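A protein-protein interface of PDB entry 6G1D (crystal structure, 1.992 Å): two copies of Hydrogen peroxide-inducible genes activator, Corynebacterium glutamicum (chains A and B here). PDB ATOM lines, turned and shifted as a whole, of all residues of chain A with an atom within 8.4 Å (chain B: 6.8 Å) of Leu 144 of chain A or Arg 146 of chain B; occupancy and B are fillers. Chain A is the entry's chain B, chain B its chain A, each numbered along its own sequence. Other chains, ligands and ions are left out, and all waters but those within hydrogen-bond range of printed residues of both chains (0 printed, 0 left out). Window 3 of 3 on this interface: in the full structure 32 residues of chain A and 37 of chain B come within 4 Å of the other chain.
OD2 of Asp 147 of chain A lies close to OD2 of Asp 147 of chain B (2.7 Å). The side-chain amino group (NZ) of Lys 139 of chain A sits close to the side-chain amino group (NZ) of Lys 139 of chain B (3.2 Å).
The backbone carbonyl oxygen of Leu 144 of chain A is in hydrogen-bond range of the backbone NH of Ile 150 of chain A, at 3.5 Å. The side-chain carboxylate of Asp 147 of chain A sits close to the backbone NH of Ala 149 of chain A, 3.2 Å away. The backbone NH (N) of Ala 149 of chain B is in hydrogen-bond range of the backbone carbonyl oxygen (O) of Leu 144 of chain B (2.9 Å). The backbone NH of Ile 150 of chain B is in hydrogen-bond range of the backbone carbonyl oxygen of Leu 144 of chain B (3.5 Å). The guanidinium group (NH2) of Arg 146 of chain B lies within salt-bridge range of the side-chain carboxylate (OD1) of Asp 147 of chain B, at 3.0 Å. The backbone carbonyl oxygen of Arg 146 of chain B lies within hydrogen-bond range of the guanidinium group of Arg 287 of chain B (3.1 Å).
Leu 144 of chain A touches Arg 146 of chain B. Asp 147 of chain B touches Leu 144 of chain A. CD2 of Leu 144 of chain B touches OD2 of Asp 147 of chain A, at 3.7 Å. CB of Asp 147 of chain A touches CB of Ala 149 of chain B, at 3.5 Å. Ala 149 of chain A touches Asp 147 of chain B.
Leu 144 of chain A touches just these residues of chain B: Arg 146 and Asp 147. Arg 146 of chain B touches just one residue of chain A: Leu 144. Printed residues of chain A within 4 Å of Asp 147 of chain B: Leu 144 (3.3 Å), Asp 147 (2.7 Å) and Ala 149 (3.7 Å). Of the printed residues of chain A, Lys 139 of chain B touches Lys 139 (3.2 Å). Of the printed residues of chain B, Asp 147 of chain A touches Leu 144, Asp 147 and Ala 149. Printed residues of chain A within 4 Å of Leu 144 of chain B: Asp 147 (3.7 Å). The nearest residue of chain B that does not touch Leu 144 of chain A is Ala 143 of chain B (6.0 Å). The nearest residue of chain A that does not touch Arg 146 of chain B is Asp 147 of chain A (5.7 Å).
Printed residues of chain A that touch a printed residue of chain B: Lys 139, Leu 144, Asp 147 and Ala 149. Hydrophobic or aromatic side chains of chain A within 4 Å of the printed part of chain B: Leu 144 and Ala 149. Among the printed residues, no Asp or Glu carboxylate lies within 4 Å of a Lys or Arg side-chain nitrogen of the other chain.
Lys 139 of chain B touches its own counterpart, Lys 139 of chain A. Leu 144 of chain A touches Arg 146 of chain B, but with the chains exchanged Arg 146 of chain A does not touch Leu 144 of chain B (6.7 Å). Leu 144 of chain A touches Asp 147 of chain B, and with the chains exchanged Asp 147 of chain A touches Leu 144 of chain B. Asp 147 of chain A touches Ala 149 of chain B, and with the chains exchanged Ala 149 of chain A touches Asp 147 of chain B. 13 positions are printed for both chains.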
ATOM      1  N   THR A 103      16.547  19.842  24.326  1.00  0.00           N
ATOM      2  CA  THR A 103      16.590  21.256  24.655  1.00  0.00           C
ATOM      3  C   THR A 103      16.121  22.036  23.435  1.00  0.00           C
ATOM      4  O   THR A 103      16.697  21.907  22.337  1.00  0.00           O
ATOM      5  CB  THR A 103      17.984  21.653  25.084  1.00  0.00           C
ATOM      6  OG1 THR A 103      18.308  20.872  26.229  1.00  0.00           O
ATOM      7  CG2 THR A 103      18.036  23.117  25.494  1.00  0.00           C
ATOM      8  N   VAL A 104      15.050  22.809  23.630  1.00  0.00           N
ATOM      9  CA  VAL A 104      14.333  23.451  22.544  1.00  0.00           C
ATOM     10  C   VAL A 104      14.444  24.956  22.771  1.00  0.00           C
ATOM     11  O   VAL A 104      14.032  25.480  23.834  1.00  0.00           O
ATOM     12  CB  VAL A 104      12.850  23.026  22.521  1.00  0.00           C
ATOM     13  CG1 VAL A 104      12.113  23.693  21.373  1.00  0.00           C
ATOM     14  CG2 VAL A 104      12.748  21.524  22.390  1.00  0.00           C
ATOM     15  N   GLY A 105      15.010  25.639  21.775  1.00  0.00           N
ATOM     16  CA  GLY A 105      15.088  27.072  21.786  1.00  0.00           C
ATOM     17  C   GLY A 105      13.808  27.588  21.134  1.00  0.00           C
ATOM     18  O   GLY A 105      13.362  27.010  20.151  1.00  0.00           O
ATOM     19  N   ILE A 106      13.226  28.663  21.679  1.00  0.00           N
ATOM     20  CA  ILE A 106      12.056  29.273  21.071  1.00  0.00           C
ATOM     21  C   ILE A 106      12.133  30.779  21.193  1.00  0.00           C
ATOM     22  O   ILE A 106      12.488  31.294  22.250  1.00  0.00           O
ATOM     23  CB  ILE A 106      10.745  28.832  21.780  1.00  0.00           C
ATOM     24  CG1 ILE A 106      10.695  27.297  21.952  1.00  0.00           C
ATOM     25  CG2 ILE A 106       9.517  29.333  20.997  1.00  0.00           C
ATOM     26  CD1 ILE A 106       9.530  26.880  22.843  1.00  0.00           C
ATOM     27  N   VAL A 134      14.605  26.982  26.220  1.00  0.00           N
ATOM     28  CA  VAL A 134      15.436  28.168  26.231  1.00  0.00           C
ATOM     29  C   VAL A 134      14.715  29.201  25.357  1.00  0.00           C
ATOM     30  O   VAL A 134      14.609  29.049  24.150  1.00  0.00           O
ATOM     31  CB  VAL A 134      16.839  27.909  25.686  1.00  0.00           C
ATOM     32  CG1 VAL A 134      17.630  29.209  25.705  1.00  0.00           C
ATOM     33  CG2 VAL A 134      17.524  26.836  26.540  1.00  0.00           C
ATOM     34  N   GLU A 135      14.207  30.254  25.995  1.00  0.00           N
ATOM     35  CA  GLU A 135      13.502  31.305  25.316  1.00  0.00           C
ATOM     36  C   GLU A 135      14.549  32.396  25.111  1.00  0.00           C
ATOM     37  O   GLU A 135      15.091  32.919  26.085  1.00  0.00           O
ATOM     38  CB  GLU A 135      12.378  31.825  26.187  1.00  0.00           C
ATOM     39  CG  GLU A 135      11.618  32.989  25.540  1.00  0.00           C
ATOM     40  CD  GLU A 135      10.517  33.575  26.419  1.00  0.00           C
ATOM     41  OE1 GLU A 135       9.457  33.764  25.801  1.00  0.00           O
ATOM     42  OE2 GLU A 135      10.676  33.833  27.644  1.00  0.00           O
ATOM     43  N   ASP A 136      14.856  32.715  23.857  1.00  0.00           N
ATOM     44  CA  ASP A 136      15.858  33.745  23.579  1.00  0.00           C
ATOM     45  C   ASP A 136      15.669  34.204  22.153  1.00  0.00           C
ATOM     46  O   ASP A 136      14.974  33.567  21.342  1.00  0.00           O
ATOM     47  CB  ASP A 136      17.298  33.214  23.806  1.00  0.00           C
ATOM     48  CG  ASP A 136      18.287  34.308  24.315  1.00  0.00           C
ATOM     49  OD1 ASP A 136      18.109  35.527  24.025  1.00  0.00           O
ATOM     50  OD2 ASP A 136      19.261  33.931  25.012  1.00  0.00           O
ATOM     51  N   GLN A 137      16.260  35.358  21.853  1.00  0.00           N
ATOM     52  CA  GLN A 137      16.181  35.949  20.514  1.00  0.00           C
ATOM     53  C   GLN A 137      16.967  35.126  19.502  1.00  0.00           C
ATOM     54  O   GLN A 137      17.857  34.345  19.848  1.00  0.00           O
ATOM     55  CB  GLN A 137      16.633  37.399  20.569  1.00  0.00           C
ATOM     56  CG  GLN A 137      15.612  38.252  21.375  1.00  0.00           C
ATOM     57  CD  GLN A 137      16.045  39.679  21.694  1.00  0.00           C
ATOM     58  OE1 GLN A 137      15.242  40.505  22.098  1.00  0.00           O
ATOM     59  NE2 GLN A 137      17.334  39.963  21.510  1.00  0.00           N
ATOM     60  N   THR A 138      16.603  35.316  18.242  1.00  0.00           N
ATOM     61  CA  THR A 138      17.016  34.488  17.129  1.00  0.00           C
ATOM     62  C   THR A 138      18.557  34.303  17.019  1.00  0.00           C
ATOM     63  O   THR A 138      19.048  33.192  16.891  1.00  0.00           O
ATOM     64  CB  THR A 138      16.441  35.094  15.837  1.00  0.00           C
ATOM     65  OG1 THR A 138      14.991  35.060  15.904  1.00  0.00           O
ATOM     66  CG2 THR A 138      16.914  34.301  14.603  1.00  0.00           C
ATOM     67  N   LYS A 139      19.289  35.408  17.079  1.00  0.00           N
ATOM     68  CA  LYS A 139      20.743  35.410  16.934  1.00  0.00           C
ATOM     69  C   LYS A 139      21.358  34.555  18.043  1.00  0.00           C
ATOM     70  O   LYS A 139      22.271  33.783  17.770  1.00  0.00           O
ATOM     71  CB  LYS A 139      21.283  36.858  16.970  1.00  0.00           C
ATOM     72  CG  LYS A 139      22.781  37.003  16.870  1.00  0.00           C
ATOM     73  CD  LYS A 139      23.254  38.455  16.948  1.00  0.00           C
ATOM     74  CE  LYS A 139      24.800  38.529  16.885  1.00  0.00           C
ATOM     75  NZ  LYS A 139      25.434  39.638  17.662  1.00  0.00           N
ATOM     76  N   HIS A 140      20.835  34.657  19.278  1.00  0.00           N
ATOM     77  CA  HIS A 140      21.314  33.816  20.353  1.00  0.00           C
ATOM     78  C   HIS A 140      20.964  32.358  20.155  1.00  0.00           C
ATOM     79  O   HIS A 140      21.810  31.491  20.405  1.00  0.00           O
ATOM     80  CB  HIS A 140      20.823  34.266  21.707  1.00  0.00           C
ATOM     81  CG  HIS A 140      21.297  35.620  22.092  1.00  0.00           C
ATOM     82  ND1 HIS A 140      20.522  36.489  22.821  1.00  0.00           N
ATOM     83  CD2 HIS A 140      22.453  36.272  21.833  1.00  0.00           C
ATOM     84  CE1 HIS A 140      21.198  37.600  23.047  1.00  0.00           C
ATOM     85  NE2 HIS A 140      22.366  37.501  22.437  1.00  0.00           N
ATOM     86  N   LEU A 141      19.737  32.069  19.700  1.00  0.00           N
ATOM     87  CA  LEU A 141      19.346  30.695  19.443  1.00  0.00           C
ATOM     88  C   LEU A 141      20.269  30.058  18.369  1.00  0.00           C
ATOM     89  O   LEU A 141      20.707  28.925  18.536  1.00  0.00           O
ATOM     90  CB  LEU A 141      17.899  30.561  19.038  1.00  0.00           C
ATOM     91  CG  LEU A 141      16.847  31.011  20.058  1.00  0.00           C
ATOM     92  CD1 LEU A 141      15.452  30.833  19.468  1.00  0.00           C
ATOM     93  CD2 LEU A 141      16.990  30.280  21.390  1.00  0.00           C
ATOM     94  N   LEU A 142      20.587  30.787  17.300  1.00  0.00           N
ATOM     95  CA  LEU A 142      21.454  30.234  16.271  1.00  0.00           C
ATOM     96  C   LEU A 142      22.882  29.970  16.812  1.00  0.00           C
ATOM     97  O   LEU A 142      23.492  28.965  16.457  1.00  0.00           O
ATOM     98  CB  LEU A 142      21.523  31.135  15.049  1.00  0.00           C
ATOM     99  CG  LEU A 142      20.240  31.191  14.220  1.00  0.00           C
ATOM    100  CD1 LEU A 142      20.287  32.374  13.244  1.00  0.00           C
ATOM    101  CD2 LEU A 142      20.000  29.883  13.469  1.00  0.00           C
ATOM    102  N   ALA A 143      23.374  30.832  17.697  1.00  0.00           N
ATOM    103  CA  ALA A 143      24.697  30.619  18.309  1.00  0.00           C
ATOM    104  C   ALA A 143      24.688  29.397  19.249  1.00  0.00           C
ATOM    105  O   ALA A 143      25.633  28.601  19.259  1.00  0.00           O
ATOM    106  CB  ALA A 143      25.151  31.878  19.054  1.00  0.00           C
ATOM    107  N   LEU A 144      23.621  29.230  20.030  1.00  0.00           N
ATOM    108  CA  LEU A 144      23.477  28.065  20.901  1.00  0.00           C
ATOM    109  C   LEU A 144      23.382  26.773  20.078  1.00  0.00           C
ATOM    110  O   LEU A 144      23.928  25.746  20.469  1.00  0.00           O
ATOM    111  CB  LEU A 144      22.238  28.206  21.822  1.00  0.00           C
ATOM    112  CG  LEU A 144      22.254  29.327  22.858  1.00  0.00           C
ATOM    113  CD1 LEU A 144      20.853  29.620  23.336  1.00  0.00           C
ATOM    114  CD2 LEU A 144      23.136  28.985  24.033  1.00  0.00           C
ATOM    115  N   LEU A 145      22.689  26.828  18.941  1.00  0.00           N
ATOM    116  CA  LEU A 145      22.618  25.689  18.037  1.00  0.00           C
ATOM    117  C   LEU A 145      24.004  25.321  17.502  1.00  0.00           C
ATOM    118  O   LEU A 145      24.366  24.163  17.492  1.00  0.00           O
ATOM    119  CB  LEU A 145      21.720  25.988  16.845  1.00  0.00           C
ATOM    120  CG  LEU A 145      20.290  25.587  16.786  1.00  0.00           C
ATOM    121  CD1 LEU A 145      19.795  26.129  15.445  1.00  0.00           C
ATOM    122  CD2 LEU A 145      20.160  24.085  16.947  1.00  0.00           C
ATOM    123  N   ARG A 146      24.764  26.315  17.050  1.00  0.00           N
ATOM    124  CA  ARG A 146      26.098  26.081  16.515  1.00  0.00           C
ATOM    125  C   ARG A 146      27.007  25.470  17.590  1.00  0.00           C
ATOM    126  O   ARG A 146      27.773  24.563  17.266  1.00  0.00           O
ATOM    127  CB  ARG A 146      26.724  27.355  15.932  1.00  0.00           C
ATOM    128  CG  ARG A 146      26.363  27.645  14.493  1.00  0.00           C
ATOM    129  CD  ARG A 146      27.082  28.894  13.981  1.00  0.00           C
ATOM    130  NE  ARG A 146      26.293  29.546  12.918  1.00  0.00           N
ATOM    131  CZ  ARG A 146      25.472  30.594  13.075  1.00  0.00           C
ATOM    132  NH1 ARG A 146      25.321  31.216  14.256  1.00  0.00           N
ATOM    133  NH2 ARG A 146      24.801  31.049  12.015  1.00  0.00           N
ATOM    134  N   ASP A 147      26.894  25.913  18.865  1.00  0.00           N
ATOM    135  CA  ASP A 147      27.775  25.371  19.912  1.00  0.00           C
ATOM    136  C   ASP A 147      27.247  24.108  20.578  1.00  0.00           C
ATOM    137  O   ASP A 147      27.897  23.580  21.459  1.00  0.00           O
ATOM    138  CB  ASP A 147      28.308  26.432  20.908  1.00  0.00           C
ATOM    139  CG  ASP A 147      27.255  27.131  21.671  1.00  0.00           C
ATOM    140  OD1 ASP A 147      26.329  26.428  22.109  1.00  0.00           O
ATOM    141  OD2 ASP A 147      27.397  28.365  21.945  1.00  0.00           O
ATOM    142  N   GLY A 148      26.082  23.629  20.154  1.00  0.00           N
ATOM    143  CA  GLY A 148      25.499  22.398  20.670  1.00  0.00           C
ATOM    144  C   GLY A 148      24.754  22.550  21.986  1.00  0.00           C
ATOM    145  O   GLY A 148      24.364  21.552  22.575  1.00  0.00           O
ATOM    146  N   ALA A 149      24.525  23.771  22.456  1.00  0.00           N
ATOM    147  CA  ALA A 149      23.897  23.994  23.758  1.00  0.00           C
ATOM    148  C   ALA A 149      22.395  23.814  23.709  1.00  0.00           C
ATOM    149  O   ALA A 149      21.775  23.613  24.760  1.00  0.00           O
ATOM    150  CB  ALA A 149      24.230  25.367  24.315  1.00  0.00           C
ATOM    151  N   ILE A 150      21.802  23.931  22.512  1.00  0.00           N
ATOM    152  CA  ILE A 150      20.437  23.460  22.291  1.00  0.00           C
ATOM    153  C   ILE A 150      20.446  22.500  21.092  1.00  0.00           C
ATOM    154  O   ILE A 150      21.368  22.554  20.254  1.00  0.00           O
ATOM    155  CB  ILE A 150      19.436  24.606  22.067  1.00  0.00           C
ATOM    156  CG1 ILE A 150      19.640  25.283  20.691  1.00  0.00           C
ATOM    157  CG2 ILE A 150      19.502  25.591  23.215  1.00  0.00           C
ATOM    158  CD1 ILE A 150      18.809  26.562  20.497  1.00  0.00           C
ATOM    159  N   ASP A 151      19.390  21.697  21.005  1.00  0.00           N
ATOM    160  CA  ASP A 151      19.215  20.721  19.942  1.00  0.00           C
ATOM    161  C   ASP A 151      18.463  21.259  18.719  1.00  0.00           C
ATOM    162  O   ASP A 151      18.811  20.975  17.559  1.00  0.00           O
ATOM    163  CB  ASP A 151      18.467  19.504  20.511  1.00  0.00           C
ATOM    164  CG  ASP A 151      19.270  18.785  21.629  1.00  0.00           C
ATOM    165  OD1 ASP A 151      20.453  18.428  21.356  1.00  0.00           O
ATOM    166  OD2 ASP A 151      18.745  18.609  22.765  1.00  0.00           O
ATOM    167  N   VAL A 152      17.392  22.009  18.986  1.00  0.00           N
ATOM    168  CA  VAL A 152      16.548  22.545  17.933  1.00  0.00           C
ATOM    169  C   VAL A 152      16.079  23.932  18.329  1.00  0.00           C
ATOM    170  O   VAL A 152      16.065  24.260  19.503  1.00  0.00           O
ATOM    171  CB  VAL A 152      15.317  21.635  17.660  1.00  0.00           C
ATOM    172  CG1 VAL A 152      15.710  20.300  17.047  1.00  0.00           C
ATOM    173  CG2 VAL A 152      14.473  21.431  18.909  1.00  0.00           C
ATOM    174  N   ALA A 153      15.679  24.733  17.348  1.00  0.00           N
ATOM    175  CA  ALA A 153      15.216  26.088  17.615  1.00  0.00           C
ATOM    176  C   ALA A 153      14.017  26.401  16.763  1.00  0.00           C
ATOM    177  O   ALA A 153      14.025  26.175  15.555  1.00  0.00           O
ATOM    178  CB  ALA A 153      16.304  27.106  17.351  1.00  0.00           C
ATOM    179  N   MET A 164      22.723  25.000   8.858  1.00  0.00           N
ATOM    180  CA  MET A 164      21.523  24.417   9.441  1.00  0.00           C
ATOM    181  C   MET A 164      20.464  23.915   8.479  1.00  0.00           C
ATOM    182  O   MET A 164      20.417  24.330   7.335  1.00  0.00           O
ATOM    183  CB  MET A 164      20.829  25.486  10.279  1.00  0.00           C
ATOM    184  CG  MET A 164      21.735  26.292  11.166  1.00  0.00           C
ATOM    185  SD  MET A 164      22.193  25.323  12.585  1.00  0.00           S
ATOM    186  CE  MET A 164      22.958  26.548  13.620  1.00  0.00           C
ATOM    187  N   ARG A 287      21.110  21.661  13.399  1.00  0.00           N
ATOM    188  CA  ARG A 287      22.432  21.519  12.722  1.00  0.00           C
ATOM    189  C   ARG A 287      22.339  20.477  11.621  1.00  0.00           C
ATOM    190  O   ARG A 287      21.879  19.368  11.865  1.00  0.00           O
ATOM    191  CB  ARG A 287      23.478  21.051  13.703  1.00  0.00           C
ATOM    192  CG  ARG A 287      23.839  22.056  14.762  1.00  0.00           C
ATOM    193  CD  ARG A 287      24.907  21.456  15.704  1.00  0.00           C
ATOM    194  NE  ARG A 287      24.402  20.334  16.508  1.00  0.00           N
ATOM    195  CZ  ARG A 287      23.616  20.430  17.573  1.00  0.00           C
ATOM    196  NH1 ARG A 287      23.192  21.630  18.021  1.00  0.00           N
ATOM    197  NH2 ARG A 287      23.209  19.320  18.187  1.00  0.00           N
ATOM    198  N   LYS B 139      31.654  39.285  24.043  1.00  0.00           N
ATOM    199  CA  LYS B 139      30.314  38.833  24.433  1.00  0.00           C
ATOM    200  C   LYS B 139      30.086  37.411  23.907  1.00  0.00           C
ATOM    201  O   LYS B 139      29.525  36.584  24.614  1.00  0.00           O
ATOM    202  CB  LYS B 139      29.220  39.818  23.982  1.00  0.00           C
ATOM    203  CG  LYS B 139      28.809  39.820  22.519  1.00  0.00           C
ATOM    204  CD  LYS B 139      27.580  40.706  22.298  1.00  0.00           C
ATOM    205  CE  LYS B 139      27.252  40.910  20.808  1.00  0.00           C
ATOM    206  NZ  LYS B 139      25.788  40.996  20.502  1.00  0.00           N
ATOM    207  N   LEU B 141      32.579  35.185  23.243  1.00  0.00           N
ATOM    208  CA  LEU B 141      33.474  34.313  24.024  1.00  0.00           C
ATOM    209  C   LEU B 141      32.849  33.992  25.388  1.00  0.00           C
ATOM    210  O   LEU B 141      32.905  32.848  25.815  1.00  0.00           O
ATOM    211  CB  LEU B 141      34.869  34.907  24.224  1.00  0.00           C
ATOM    212  CG  LEU B 141      35.668  35.139  22.933  1.00  0.00           C
ATOM    213  CD1 LEU B 141      37.001  35.759  23.292  1.00  0.00           C
ATOM    214  CD2 LEU B 141      35.863  33.858  22.126  1.00  0.00           C
ATOM    215  N   LEU B 142      32.234  34.969  26.058  1.00  0.00           N
ATOM    216  CA  LEU B 142      31.605  34.684  27.353  1.00  0.00           C
ATOM    217  C   LEU B 142      30.431  33.711  27.214  1.00  0.00           C
ATOM    218  O   LEU B 142      30.262  32.850  28.050  1.00  0.00           O
ATOM    219  CB  LEU B 142      31.168  35.961  28.061  1.00  0.00           C
ATOM    220  CG  LEU B 142      32.308  36.840  28.571  1.00  0.00           C
ATOM    221  CD1 LEU B 142      31.794  38.237  28.906  1.00  0.00           C
ATOM    222  CD2 LEU B 142      33.043  36.170  29.742  1.00  0.00           C
ATOM    223  N   ALA B 143      29.669  33.813  26.134  1.00  0.00           N
ATOM    224  CA  ALA B 143      28.563  32.873  25.868  1.00  0.00           C
ATOM    225  C   ALA B 143      29.086  31.459  25.582  1.00  0.00           C
ATOM    226  O   ALA B 143      28.545  30.484  26.073  1.00  0.00           O
ATOM    227  CB  ALA B 143      27.681  33.376  24.731  1.00  0.00           C
ATOM    228  N   LEU B 144      30.164  31.349  24.800  1.00  0.00           N
ATOM    229  CA  LEU B 144      30.796  30.060  24.524  1.00  0.00           C
ATOM    230  C   LEU B 144      31.349  29.428  25.825  1.00  0.00           C
ATOM    231  O   LEU B 144      31.261  28.226  26.027  1.00  0.00           O
ATOM    232  CB  LEU B 144      31.900  30.206  23.462  1.00  0.00           C
ATOM    233  CG  LEU B 144      31.470  30.611  22.048  1.00  0.00           C
ATOM    234  CD1 LEU B 144      32.620  31.151  21.238  1.00  0.00           C
ATOM    235  CD2 LEU B 144      30.834  29.468  21.283  1.00  0.00           C
ATOM    236  N   LEU B 145      31.920  30.248  26.695  1.00  0.00           N
ATOM    237  CA  LEU B 145      32.418  29.775  27.989  1.00  0.00           C
ATOM    238  C   LEU B 145      31.259  29.242  28.847  1.00  0.00           C
ATOM    239  O   LEU B 145      31.358  28.179  29.450  1.00  0.00           O
ATOM    240  CB  LEU B 145      33.086  30.901  28.762  1.00  0.00           C
ATOM    241  CG  LEU B 145      34.568  31.105  28.763  1.00  0.00           C
ATOM    242  CD1 LEU B 145      34.803  32.318  29.640  1.00  0.00           C
ATOM    243  CD2 LEU B 145      35.313  29.862  29.266  1.00  0.00           C
ATOM    244  N   ARG B 146      30.162  29.983  28.909  1.00  0.00           N
ATOM    245  CA  ARG B 146      28.992  29.549  29.684  1.00  0.00           C
ATOM    246  C   ARG B 146      28.423  28.248  29.143  1.00  0.00           C
ATOM    247  O   ARG B 146      28.025  27.416  29.930  1.00  0.00           O
ATOM    248  CB  ARG B 146      27.943  30.681  29.740  1.00  0.00           C
ATOM    249  CG  ARG B 146      26.609  30.491  30.427  1.00  0.00           C
ATOM    250  CD  ARG B 146      25.617  31.479  29.806  1.00  0.00           C
ATOM    251  NE  ARG B 146      25.343  31.029  28.428  1.00  0.00           N
ATOM    252  CZ  ARG B 146      24.990  31.801  27.395  1.00  0.00           C
ATOM    253  NH1 ARG B 146      24.782  33.118  27.526  1.00  0.00           N
ATOM    254  NH2 ARG B 146      24.816  31.234  26.202  1.00  0.00           N
ATOM    255  N   ASP B 147      28.430  28.038  27.825  1.00  0.00           N
ATOM    256  CA  ASP B 147      27.883  26.802  27.202  1.00  0.00           C
ATOM    257  C   ASP B 147      28.870  25.642  27.203  1.00  0.00           C
ATOM    258  O   ASP B 147      28.509  24.533  26.828  1.00  0.00           O
ATOM    259  CB  ASP B 147      27.477  27.027  25.733  1.00  0.00           C
ATOM    260  CG  ASP B 147      26.419  28.108  25.547  1.00  0.00           C
ATOM    261  OD1 ASP B 147      25.616  28.346  26.475  1.00  0.00           O
ATOM    262  OD2 ASP B 147      26.423  28.734  24.460  1.00  0.00           O
ATOM    263  N   GLY B 148      30.109  25.887  27.598  1.00  0.00           N
ATOM    264  CA  GLY B 148      31.156  24.858  27.586  1.00  0.00           C
ATOM    265  C   GLY B 148      31.807  24.634  26.230  1.00  0.00           C
ATOM    266  O   GLY B 148      32.567  23.702  26.073  1.00  0.00           O
ATOM    267  N   ALA B 149      31.538  25.483  25.251  1.00  0.00           N
ATOM    268  CA  ALA B 149      32.055  25.286  23.892  1.00  0.00           C
ATOM    269  C   ALA B 149      33.508  25.729  23.764  1.00  0.00           C
ATOM    270  O   ALA B 149      34.142  25.352  22.803  1.00  0.00           O
ATOM    271  CB  ALA B 149      31.194  26.030  22.861  1.00  0.00           C
ATOM    272  N   ILE B 150      33.978  26.582  24.674  1.00  0.00           N
ATOM    273  CA  ILE B 150      35.399  26.797  24.877  1.00  0.00           C
ATOM    274  C   ILE B 150      35.734  26.607  26.344  1.00  0.00           C
ATOM    275  O   ILE B 150      34.866  26.693  27.205  1.00  0.00           O
ATOM    276  CB  ILE B 150      35.885  28.196  24.394  1.00  0.00           C
ATOM    277  CG1 ILE B 150      35.386  29.314  25.332  1.00  0.00           C
ATOM    278  CG2 ILE B 150      35.473  28.440  22.951  1.00  0.00           C
ATOM    279  CD1 ILE B 150      35.644  30.705  24.841  1.00  0.00           C
ATOM    280  N   MET B 164      32.412  33.388  36.436  1.00  0.00           N
ATOM    281  CA  MET B 164      33.738  33.226  35.856  1.00  0.00           C
ATOM    282  C   MET B 164      34.840  33.527  36.865  1.00  0.00           C
ATOM    283  O   MET B 164      34.642  34.331  37.764  1.00  0.00           O
ATOM    284  CB  MET B 164      33.892  34.140  34.645  1.00  0.00           C
ATOM    285  CG  MET B 164      32.861  33.922  33.545  1.00  0.00           C
ATOM    286  SD  MET B 164      32.817  32.221  32.926  1.00  0.00           S
ATOM    287  CE  MET B 164      31.502  32.400  31.747  1.00  0.00           C
ATOM    288  N   ARG B 287      35.346  29.192  33.573  1.00  0.00           N
ATOM    289  CA  ARG B 287      34.182  28.893  34.467  1.00  0.00           C
ATOM    290  C   ARG B 287      34.657  28.578  35.880  1.00  0.00           C
ATOM    291  O   ARG B 287      35.523  27.727  36.056  1.00  0.00           O
ATOM    292  CB  ARG B 287      33.419  27.689  33.971  1.00  0.00           C
ATOM    293  CG  ARG B 287      32.706  27.865  32.669  1.00  0.00           C
ATOM    294  CD  ARG B 287      32.345  26.488  32.098  1.00  0.00           C
ATOM    295  NE  ARG B 287      30.913  26.244  32.076  1.00  0.00           N
ATOM    296  CZ  ARG B 287      30.345  25.143  31.588  1.00  0.00           C
ATOM    297  NH1 ARG B 287      31.079  24.109  31.128  1.00  0.00           N
ATOM    298  NH2 ARG B 287      29.019  25.019  31.615  1.00  0.00           N
